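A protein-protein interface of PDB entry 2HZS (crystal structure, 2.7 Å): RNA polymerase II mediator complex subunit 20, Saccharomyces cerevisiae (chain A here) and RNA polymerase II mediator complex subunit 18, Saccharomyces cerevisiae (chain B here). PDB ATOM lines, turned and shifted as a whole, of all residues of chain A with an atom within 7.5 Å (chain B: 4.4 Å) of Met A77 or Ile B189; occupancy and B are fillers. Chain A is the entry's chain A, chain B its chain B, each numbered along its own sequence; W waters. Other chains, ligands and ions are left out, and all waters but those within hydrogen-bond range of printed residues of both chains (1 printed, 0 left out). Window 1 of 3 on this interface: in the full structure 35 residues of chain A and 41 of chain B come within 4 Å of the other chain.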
ATOM      1  N   TYR A  57      -0.816  16.549 -21.009  1.00  0.00           N
ATOM      2  CA  TYR A  57      -1.933  15.669 -21.333  1.00  0.00           C
ATOM      3  C   TYR A  57      -3.067  15.795 -20.319  1.00  0.00           C
ATOM      4  O   TYR A  57      -2.832  16.009 -19.125  1.00  0.00           O
ATOM      5  CB  TYR A  57      -1.447  14.219 -21.419  1.00  0.00           C
ATOM      6  CG  TYR A  57      -0.330  14.045 -22.420  1.00  0.00           C
ATOM      7  CD1 TYR A  57       1.005  14.120 -22.023  1.00  0.00           C
ATOM      8  CD2 TYR A  57      -0.609  13.906 -23.784  1.00  0.00           C
ATOM      9  CE1 TYR A  57       2.030  14.066 -22.956  1.00  0.00           C
ATOM     10  CE2 TYR A  57       0.401  13.858 -24.728  1.00  0.00           C
ATOM     11  CZ  TYR A  57       1.721  13.939 -24.313  1.00  0.00           C
ATOM     12  OH  TYR A  57       2.733  13.905 -25.257  1.00  0.00           O
ATOM     13  N   ILE A  59      -6.426  13.649 -19.170  1.00  0.00           N
ATOM     14  CA  ILE A  59      -7.179  12.392 -19.260  1.00  0.00           C
ATOM     15  C   ILE A  59      -8.490  12.477 -18.470  1.00  0.00           C
ATOM     16  O   ILE A  59      -8.477  12.510 -17.233  1.00  0.00           O
ATOM     17  CB  ILE A  59      -6.376  11.183 -18.686  1.00  0.00           C
ATOM     18  CG1 ILE A  59      -5.020  11.056 -19.381  1.00  0.00           C
ATOM     19  CG2 ILE A  59      -7.178   9.895 -18.858  1.00  0.00           C
ATOM     20  CD1 ILE A  59      -3.991  12.034 -18.896  1.00  0.00           C
ATOM     21  N   THR A  68     -10.775  14.602 -14.141  1.00  0.00           N
ATOM     22  CA  THR A  68      -9.786  14.825 -15.173  1.00  0.00           C
ATOM     23  C   THR A  68      -8.418  14.971 -14.536  1.00  0.00           C
ATOM     24  O   THR A  68      -8.224  15.768 -13.625  1.00  0.00           O
ATOM     25  CB  THR A  68     -10.105  16.076 -15.993  1.00  0.00           C
ATOM     26  OG1 THR A  68     -11.379  15.920 -16.626  1.00  0.00           O
ATOM     27  CG2 THR A  68      -9.042  16.292 -17.057  1.00  0.00           C
ATOM     28  N   VAL A  69      -7.478  14.168 -15.009  1.00  0.00           N
ATOM     29  CA  VAL A  69      -6.124  14.213 -14.500  1.00  0.00           C
ATOM     30  C   VAL A  69      -5.216  14.925 -15.499  1.00  0.00           C
ATOM     31  O   VAL A  69      -5.211  14.597 -16.692  1.00  0.00           O
ATOM     32  CB  VAL A  69      -5.566  12.790 -14.262  1.00  0.00           C
ATOM     33  CG1 VAL A  69      -4.154  12.864 -13.720  1.00  0.00           C
ATOM     34  CG2 VAL A  69      -6.483  12.011 -13.310  1.00  0.00           C
ATOM     35  N   LEU A  70      -4.481  15.926 -15.021  1.00  0.00           N
ATOM     36  CA  LEU A  70      -3.534  16.626 -15.881  1.00  0.00           C
ATOM     37  C   LEU A  70      -2.143  16.029 -15.660  1.00  0.00           C
ATOM     38  O   LEU A  70      -1.729  15.804 -14.523  1.00  0.00           O
ATOM     39  CB  LEU A  70      -3.499  18.121 -15.582  1.00  0.00           C
ATOM     40  CG  LEU A  70      -4.443  18.949 -16.452  1.00  0.00           C
ATOM     41  CD1 LEU A  70      -5.643  19.422 -15.632  1.00  0.00           C
ATOM     42  CD2 LEU A  70      -3.647  20.093 -17.005  1.00  0.00           C
ATOM     43  N   ILE A  71      -1.441  15.737 -16.748  1.00  0.00           N
ATOM     44  CA  ILE A  71      -0.114  15.170 -16.635  1.00  0.00           C
ATOM     45  C   ILE A  71       0.898  15.932 -17.469  1.00  0.00           C
ATOM     46  O   ILE A  71       0.722  16.117 -18.679  1.00  0.00           O
ATOM     47  CB  ILE A  71      -0.101  13.676 -17.039  1.00  0.00           C
ATOM     48  CG1 ILE A  71      -0.894  12.870 -16.012  1.00  0.00           C
ATOM     49  CG2 ILE A  71       1.330  13.167 -17.138  1.00  0.00           C
ATOM     50  CD1 ILE A  71      -0.521  11.433 -15.941  1.00  0.00           C
ATOM     51  N   LYS A  72       1.947  16.385 -16.794  1.00  0.00           N
ATOM     52  CA  LYS A  72       3.032  17.129 -17.419  1.00  0.00           C
ATOM     53  C   LYS A  72       4.343  16.901 -16.654  1.00  0.00           C
ATOM     54  O   LYS A  72       4.367  16.949 -15.421  1.00  0.00           O
ATOM     55  CB  LYS A  72       2.708  18.624 -17.459  1.00  0.00           C
ATOM     56  CG  LYS A  72       3.837  19.466 -18.024  1.00  0.00           C
ATOM     57  CD  LYS A  72       3.451  20.926 -18.168  1.00  0.00           C
ATOM     58  CE  LYS A  72       4.688  21.803 -18.345  1.00  0.00           C
ATOM     59  NZ  LYS A  72       5.524  21.381 -19.501  1.00  0.00           N
ATOM     60  N   SER A  75       4.380  14.557 -13.669  1.00  0.00           N
ATOM     61  CA  SER A  75       3.655  15.009 -12.494  1.00  0.00           C
ATOM     62  C   SER A  75       2.189  15.049 -12.872  1.00  0.00           C
ATOM     63  O   SER A  75       1.851  15.299 -14.031  1.00  0.00           O
ATOM     64  CB  SER A  75       4.160  16.377 -12.055  1.00  0.00           C
ATOM     65  OG  SER A  75       5.458  16.244 -11.501  1.00  0.00           O
ATOM     66  N   ALA A  76       1.325  14.780 -11.899  1.00  0.00           N
ATOM     67  CA  ALA A  76      -0.110  14.742 -12.148  1.00  0.00           C
ATOM     68  C   ALA A  76      -0.957  15.552 -11.182  1.00  0.00           C
ATOM     69  O   ALA A  76      -0.652  15.664  -9.991  1.00  0.00           O
ATOM     70  CB  ALA A  76      -0.577  13.298 -12.137  1.00  0.00           C
ATOM     71  N   MET A  77      -2.033  16.113 -11.715  1.00  0.00           N
ATOM     72  CA  MET A  77      -2.983  16.891 -10.925  1.00  0.00           C
ATOM     73  C   MET A  77      -4.374  16.316 -11.200  1.00  0.00           C
ATOM     74  O   MET A  77      -4.819  16.294 -12.352  1.00  0.00           O
ATOM     75  CB  MET A  77      -2.960  18.369 -11.334  1.00  0.00           C
ATOM     76  CG  MET A  77      -3.897  19.253 -10.512  1.00  0.00           C
ATOM     77  SD  MET A  77      -4.285  20.790 -11.362  1.00  0.00           S
ATOM     78  CE  MET A  77      -3.185  21.886 -10.607  1.00  0.00           C
ATOM     79  N   VAL A  78      -5.046  15.856 -10.148  1.00  0.00           N
ATOM     80  CA  VAL A  78      -6.385  15.290 -10.272  1.00  0.00           C
ATOM     81  C   VAL A  78      -7.435  16.368 -10.049  1.00  0.00           C
ATOM     82  O   VAL A  78      -7.440  17.021  -9.007  1.00  0.00           O
ATOM     83  CB  VAL A  78      -6.642  14.185  -9.220  1.00  0.00           C
ATOM     84  CG1 VAL A  78      -8.016  13.575  -9.438  1.00  0.00           C
ATOM     85  CG2 VAL A  78      -5.555  13.125  -9.285  1.00  0.00           C
ATOM     86  N   THR A  79      -8.324  16.562 -11.016  1.00  0.00           N
ATOM     87  CA  THR A  79      -9.387  17.548 -10.846  1.00  0.00           C
ATOM     88  C   THR A  79     -10.763  16.935 -11.106  1.00  0.00           C
ATOM     89  O   THR A  79     -10.879  15.870 -11.705  1.00  0.00           O
ATOM     90  CB  THR A  79      -9.223  18.746 -11.796  1.00  0.00           C
ATOM     91  OG1 THR A  79      -9.613  18.369 -13.127  1.00  0.00           O
ATOM     92  CG2 THR A  79      -7.778  19.221 -11.791  1.00  0.00           C
ATOM     93  N   THR A  80     -11.805  17.614 -10.650  1.00  0.00           N
ATOM     94  CA  THR A  80     -13.157  17.139 -10.864  1.00  0.00           C
ATOM     95  C   THR A  80     -14.085  18.288 -11.212  1.00  0.00           C
ATOM     96  O   THR A  80     -13.906  19.411 -10.746  1.00  0.00           O
ATOM     97  CB  THR A  80     -13.707  16.428  -9.632  1.00  0.00           C
ATOM     98  OG1 THR A  80     -15.066  16.053  -9.885  1.00  0.00           O
ATOM     99  CG2 THR A  80     -13.654  17.339  -8.422  1.00  0.00           C
ATOM    100  N   PRO A  87     -15.179  18.525  -1.667  1.00  0.00           N
ATOM    101  CA  PRO A  87     -15.033  18.247  -0.236  1.00  0.00           C
ATOM    102  C   PRO A  87     -16.022  19.151   0.497  1.00  0.00           C
ATOM    103  O   PRO A  87     -16.059  20.360   0.265  1.00  0.00           O
ATOM    104  CB  PRO A  87     -13.591  18.640   0.035  1.00  0.00           C
ATOM    105  CG  PRO A  87     -12.916  18.245  -1.235  1.00  0.00           C
ATOM    106  CD  PRO A  87     -13.870  18.718  -2.311  1.00  0.00           C
ATOM    107  N   LEU A  90     -15.007  22.697   1.780  1.00  0.00           N
ATOM    108  CA  LEU A  90     -14.788  23.782   0.831  1.00  0.00           C
ATOM    109  C   LEU A  90     -16.076  24.467   0.435  1.00  0.00           C
ATOM    110  O   LEU A  90     -16.059  25.628   0.029  1.00  0.00           O
ATOM    111  CB  LEU A  90     -14.071  23.294  -0.430  1.00  0.00           C
ATOM    112  CG  LEU A  90     -12.609  22.887  -0.265  1.00  0.00           C
ATOM    113  CD1 LEU A  90     -12.080  22.404  -1.597  1.00  0.00           C
ATOM    114  CD2 LEU A  90     -11.787  24.041   0.243  1.00  0.00           C
ATOM    115  N   ILE A 103     -11.632  21.311 -16.011  1.00  0.00           N
ATOM    116  CA  ILE A 103     -10.341  21.989 -16.114  1.00  0.00           C
ATOM    117  C   ILE A 103     -10.049  22.244 -17.596  1.00  0.00           C
ATOM    118  O   ILE A 103      -9.369  23.209 -17.935  1.00  0.00           O
ATOM    119  CB  ILE A 103      -9.206  21.138 -15.507  1.00  0.00           C
ATOM    120  CG1 ILE A 103      -7.876  21.856 -15.672  1.00  0.00           C
ATOM    121  CG2 ILE A 103      -9.156  19.769 -16.163  1.00  0.00           C
ATOM    122  CD1 ILE A 103      -7.772  23.157 -14.915  1.00  0.00           C
ATOM    123  N   LEU A 188       4.173   6.920 -11.326  1.00  0.00           N
ATOM    124  CA  LEU A 188       4.732   8.237 -11.040  1.00  0.00           C
ATOM    125  C   LEU A 188       5.352   8.217  -9.650  1.00  0.00           C
ATOM    126  O   LEU A 188       4.818   7.594  -8.733  1.00  0.00           O
ATOM    127  CB  LEU A 188       3.640   9.309 -11.092  1.00  0.00           C
ATOM    128  CG  LEU A 188       2.982   9.601 -12.441  1.00  0.00           C
ATOM    129  CD1 LEU A 188       1.804  10.537 -12.244  1.00  0.00           C
ATOM    130  CD2 LEU A 188       4.000  10.207 -13.378  1.00  0.00           C
ATOM    131  N   ASN A 194      -1.742   6.765  -5.021  1.00  0.00           N
ATOM    132  CA  ASN A 194      -2.855   7.427  -5.700  1.00  0.00           C
ATOM    133  C   ASN A 194      -3.126   6.788  -7.065  1.00  0.00           C
ATOM    134  O   ASN A 194      -2.567   7.200  -8.083  1.00  0.00           O
ATOM    135  CB  ASN A 194      -2.541   8.917  -5.867  1.00  0.00           C
ATOM    136  CG  ASN A 194      -3.713   9.704  -6.407  1.00  0.00           C
ATOM    137  OD1 ASN A 194      -3.642  10.926  -6.546  1.00  0.00           O
ATOM    138  ND2 ASN A 194      -4.806   9.007  -6.712  1.00  0.00           N
ATOM    139  N   ILE A 196      -5.707   6.647  -9.502  1.00  0.00           N
ATOM    140  CA  ILE A 196      -6.116   7.442 -10.656  1.00  0.00           C
ATOM    141  C   ILE A 196      -4.955   8.109 -11.396  1.00  0.00           C
ATOM    142  O   ILE A 196      -5.009   8.295 -12.612  1.00  0.00           O
ATOM    143  CB  ILE A 196      -7.143   8.533 -10.242  1.00  0.00           C
ATOM    144  CG1 ILE A 196      -7.893   9.035 -11.471  1.00  0.00           C
ATOM    145  CG2 ILE A 196      -6.441   9.700  -9.569  1.00  0.00           C
ATOM    146  CD1 ILE A 196      -8.802   8.004 -12.076  1.00  0.00           C
ATOM    147  N   CYS A 197      -3.904   8.466 -10.670  1.00  0.00           N
ATOM    148  CA  CYS A 197      -2.760   9.121 -11.289  1.00  0.00           C
ATOM    149  C   CYS A 197      -1.900   8.209 -12.164  1.00  0.00           C
ATOM    150  O   CYS A 197      -1.533   8.586 -13.280  1.00  0.00           O
ATOM    151  CB  CYS A 197      -1.905   9.786 -10.218  1.00  0.00           C
ATOM    152  SG  CYS A 197      -2.608  11.327  -9.632  1.00  0.00           S
ATOM    153  N   ALA A 200      -3.833   7.231 -15.241  1.00  0.00           N
ATOM    154  CA  ALA A 200      -3.785   8.334 -16.196  1.00  0.00           C
ATOM    155  C   ALA A 200      -2.430   8.364 -16.881  1.00  0.00           C
ATOM    156  O   ALA A 200      -2.339   8.549 -18.095  1.00  0.00           O
ATOM    157  CB  ALA A 200      -4.029   9.647 -15.485  1.00  0.00           C
ATOM    158  N   CYS B 160      -0.591  17.414  -2.825  1.00  0.00           N
ATOM    159  CA  CYS B 160      -1.255  18.671  -2.482  1.00  0.00           C
ATOM    160  C   CYS B 160      -2.615  18.440  -1.856  1.00  0.00           C
ATOM    161  O   CYS B 160      -3.216  17.383  -2.029  1.00  0.00           O
ATOM    162  CB  CYS B 160      -1.430  19.555  -3.716  1.00  0.00           C
ATOM    163  SG  CYS B 160      -2.742  19.076  -4.863  1.00  0.00           S
ATOM    164  N   SER B 161      -3.095  19.431  -1.116  1.00  0.00           N
ATOM    165  CA  SER B 161      -4.410  19.353  -0.493  1.00  0.00           C
ATOM    166  C   SER B 161      -5.465  19.713  -1.534  1.00  0.00           C
ATOM    167  O   SER B 161      -5.145  20.178  -2.630  1.00  0.00           O
ATOM    168  CB  SER B 161      -4.527  20.361   0.644  1.00  0.00           C
ATOM    169  OG  SER B 161      -3.429  20.272   1.517  1.00  0.00           O
ATOM    170  N   PRO B 162      -6.744  19.484  -1.215  1.00  0.00           N
ATOM    171  CA  PRO B 162      -7.725  19.859  -2.238  1.00  0.00           C
ATOM    172  C   PRO B 162      -7.775  21.402  -2.280  1.00  0.00           C
ATOM    173  O   PRO B 162      -7.536  22.074  -1.273  1.00  0.00           O
ATOM    174  CB  PRO B 162      -9.024  19.259  -1.703  1.00  0.00           C
ATOM    175  CG  PRO B 162      -8.568  18.138  -0.832  1.00  0.00           C
ATOM    176  CD  PRO B 162      -7.364  18.694  -0.138  1.00  0.00           C
ATOM    177  N   TRP B 163      -8.062  21.966  -3.441  1.00  0.00           N
ATOM    178  CA  TRP B 163      -8.162  23.409  -3.566  1.00  0.00           C
ATOM    179  C   TRP B 163      -9.278  23.711  -4.537  1.00  0.00           C
ATOM    180  O   TRP B 163      -9.675  22.873  -5.342  1.00  0.00           O
ATOM    181  CB  TRP B 163      -6.890  24.047  -4.162  1.00  0.00           C
ATOM    182  CG  TRP B 163      -5.672  24.038  -3.313  1.00  0.00           C
ATOM    183  CD1 TRP B 163      -4.751  23.039  -3.214  1.00  0.00           C
ATOM    184  CD2 TRP B 163      -5.248  25.069  -2.412  1.00  0.00           C
ATOM    185  NE1 TRP B 163      -3.779  23.382  -2.305  1.00  0.00           N
ATOM    186  CE2 TRP B 163      -4.060  24.623  -1.796  1.00  0.00           C
ATOM    187  CE3 TRP B 163      -5.757  26.327  -2.065  1.00  0.00           C
ATOM    188  CZ2 TRP B 163      -3.370  25.389  -0.849  1.00  0.00           C
ATOM    189  CZ3 TRP B 163      -5.069  27.088  -1.125  1.00  0.00           C
ATOM    190  CH2 TRP B 163      -3.889  26.614  -0.529  1.00  0.00           C
ATOM    191  N   LEU B 165     -10.096  26.073  -7.641  1.00  0.00           N
ATOM    192  CA  LEU B 165      -9.381  26.923  -8.592  1.00  0.00           C
ATOM    193  C   LEU B 165     -10.403  27.788  -9.315  1.00  0.00           C
ATOM    194  O   LEU B 165     -11.334  27.279  -9.931  1.00  0.00           O
ATOM    195  CB  LEU B 165      -8.573  26.070  -9.581  1.00  0.00           C
ATOM    196  CG  LEU B 165      -7.697  26.793 -10.602  1.00  0.00           C
ATOM    197  CD1 LEU B 165      -6.639  25.840 -11.148  1.00  0.00           C
ATOM    198  CD2 LEU B 165      -8.556  27.330 -11.722  1.00  0.00           C
ATOM    199  N   THR B 187     -12.893  25.001 -10.972  1.00  0.00           N
ATOM    200  CA  THR B 187     -12.692  23.578 -11.075  1.00  0.00           C
ATOM    201  C   THR B 187     -12.120  23.207  -9.724  1.00  0.00           C
ATOM    202  O   THR B 187     -11.701  24.090  -8.981  1.00  0.00           O
ATOM    203  CB  THR B 187     -11.715  23.188 -12.177  1.00  0.00           C
ATOM    204  OG1 THR B 187     -11.708  21.769 -12.284  1.00  0.00           O
ATOM    205  CG2 THR B 187     -10.311  23.644 -11.856  1.00  0.00           C
ATOM    206  N   ILE B 188     -12.117  21.920  -9.393  1.00  0.00           N
ATOM    207  CA  ILE B 188     -11.597  21.486  -8.099  1.00  0.00           C
ATOM    208  C   ILE B 188     -10.334  20.643  -8.207  1.00  0.00           C
ATOM    209  O   ILE B 188     -10.285  19.702  -8.979  1.00  0.00           O
ATOM    210  CB  ILE B 188     -12.630  20.636  -7.324  1.00  0.00           C
ATOM    211  CG1 ILE B 188     -13.940  21.394  -7.156  1.00  0.00           C
ATOM    212  CG2 ILE B 188     -12.047  20.236  -5.974  1.00  0.00           C
ATOM    213  CD1 ILE B 188     -13.870  22.667  -6.319  1.00  0.00           C
ATOM    214  N   ILE B 189      -9.314  20.980  -7.436  1.00  0.00           N
ATOM    215  CA  ILE B 189      -8.099  20.186  -7.431  1.00  0.00           C
ATOM    216  C   ILE B 189      -8.248  19.218  -6.258  1.00  0.00           C
ATOM    217  O   ILE B 189      -8.442  19.650  -5.114  1.00  0.00           O
ATOM    218  CB  ILE B 189      -6.861  21.049  -7.196  1.00  0.00           C
ATOM    219  CG1 ILE B 189      -6.652  21.997  -8.383  1.00  0.00           C
ATOM    220  CG2 ILE B 189      -5.647  20.164  -6.991  1.00  0.00           C
ATOM    221  CD1 ILE B 189      -5.608  23.059  -8.115  1.00  0.00           C
ATOM    222  N   LEU B 190      -8.159  17.914  -6.525  1.00  0.00           N
ATOM    223  CA  LEU B 190      -8.314  16.926  -5.463  1.00  0.00           C
ATOM    224  C   LEU B 190      -7.024  16.397  -4.915  1.00  0.00           C
ATOM    225  O   LEU B 190      -6.918  16.145  -3.719  1.00  0.00           O
ATOM    226  CB  LEU B 190      -9.143  15.740  -5.942  1.00  0.00           C
ATOM    227  CG  LEU B 190     -10.619  16.025  -6.185  1.00  0.00           C
ATOM    228  CD1 LEU B 190     -11.269  14.782  -6.734  1.00  0.00           C
ATOM    229  CD2 LEU B 190     -11.273  16.465  -4.901  1.00  0.00           C
ATOM    230  N   SER B 191      -6.040  16.203  -5.780  1.00  0.00           N
ATOM    231  CA  SER B 191      -4.763  15.675  -5.332  1.00  0.00           C
ATOM    232  C   SER B 191      -3.714  15.761  -6.437  1.00  0.00           C
ATOM    233  O   SER B 191      -4.007  16.221  -7.547  1.00  0.00           O
ATOM    234  CB  SER B 191      -4.937  14.221  -4.910  1.00  0.00           C
ATOM    235  OG  SER B 191      -5.364  13.457  -6.029  1.00  0.00           O
ATOM    236  N   LEU B 202       2.729  22.740  -9.584  1.00  0.00           N
ATOM    237  CA  LEU B 202       1.634  22.543 -10.530  1.00  0.00           C
ATOM    238  C   LEU B 202       1.190  23.855 -11.179  1.00  0.00           C
ATOM    239  O   LEU B 202       0.895  23.902 -12.381  1.00  0.00           O
ATOM    240  CB  LEU B 202       0.461  21.854  -9.825  1.00  0.00           C
ATOM    241  CG  LEU B 202       0.779  20.431  -9.347  1.00  0.00           C
ATOM    242  CD1 LEU B 202      -0.382  19.857  -8.550  1.00  0.00           C
ATOM    243  CD2 LEU B 202       1.077  19.549 -10.565  1.00  0.00           C
HETATM  244  O   HOH W   1     -11.789  19.446 -14.462  1.00  0.00           O
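The backbone NH (N) of Leu B190 is in hydrogen-bond range of the backbone carbonyl oxygen (O) of Val A78, 2.7 Å away.
The backbone carbonyl oxygen (O) of Ser B191 is in hydrogen-bond range of the backbone NH (N) of Val A78 (2.8 Å).
The backbone carbonyl oxygen (O) of Ile B188 lies within hydrogen-bond range of the backbone NH (N) of Thr A80, 3.1 Å away.
OG of Ser B191 lies within hydrogen-bond range of OD1 of Asn A194 (3.1 Å).
The backbone NH (N) of Thr A79 sits at hydrogen-bond distance from the backbone carbonyl oxygen (O) of Thr A68, 2.7 Å away.
N of Leu A70 is in hydrogen-bond range of O of Met A77 (2.7 Å).
The side-chain amide oxygen (OD1) of Asn A194 sits at hydrogen-bond distance from the side-chain sulfur (SG) of Cys A197, 3.3 Å away.
O of Trp B163 lies within hydrogen-bond range of N of Ile B189, at 2.8 Å.
The backbone NH of Leu B165 lies within hydrogen-bond range of the backbone carbonyl oxygen of Thr B187 (2.9 Å).
Among the printed residues, pairs that only touch across the chains: Met A77 with Ile B189, Met A77 with Ser B191, Met A77 with Leu B202, Val A78 with Ile B188, Val A78 with Ile B189, Thr A79 with Thr B187, Thr A79 with Ile B188, Thr A80 with Thr B187, Thr A80 with Leu B190 and Ile A103 with Thr B187.
Ile A71 touches none of the printed residues of chain B.
Of the printed residues of chain B, Met A77 touches Ile B189 (3.7 Å), Ser B191 (3.6 Å) and Leu B202 (3.7 Å).
Leu A90 touches none of the printed residues of chain B.
Printed residues of chain A within 4 Å of Thr B187: Thr A79 (3.9 Å), Thr A80 (3.6 Å) and Ile A103 (3.8 Å).
Printed residues of chain A within 4 Å of Ile B188: Val A78, Thr A79 and Thr A80.
Of chain A, only Met A77 and Val A78 come within 4 Å of Ile B189.
Of the printed residues of chain A, Leu B190 touches Val A78 (2.7 Å) and Thr A80 (3.9 Å).
Of the printed residues of chain A, Leu B202 touches Met A77.
The nearest residue of chain A that does not touch Ile B189 is Thr A79 (4.5 Å).
Along chain A the printed residues that touch a printed residue of chain B span positions 77 to 194.
Of the 11 printed residues of chain B, 6 touch a printed residue of chain A.
Hydrophobic or aromatic side chains of chain B within 4 Å of the printed part of chain A: Ile B188, Ile B189, Leu B190 and Leu B202.
Water W1 lies within hydrogen-bond range of the backbone NH (N) of Ile A103 (2.4 Å), the side-chain hydroxyl (OG1) of Thr A79 (2.8 Å) and the side-chain hydroxyl (OG1) of Thr B187 (3.2 Å).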
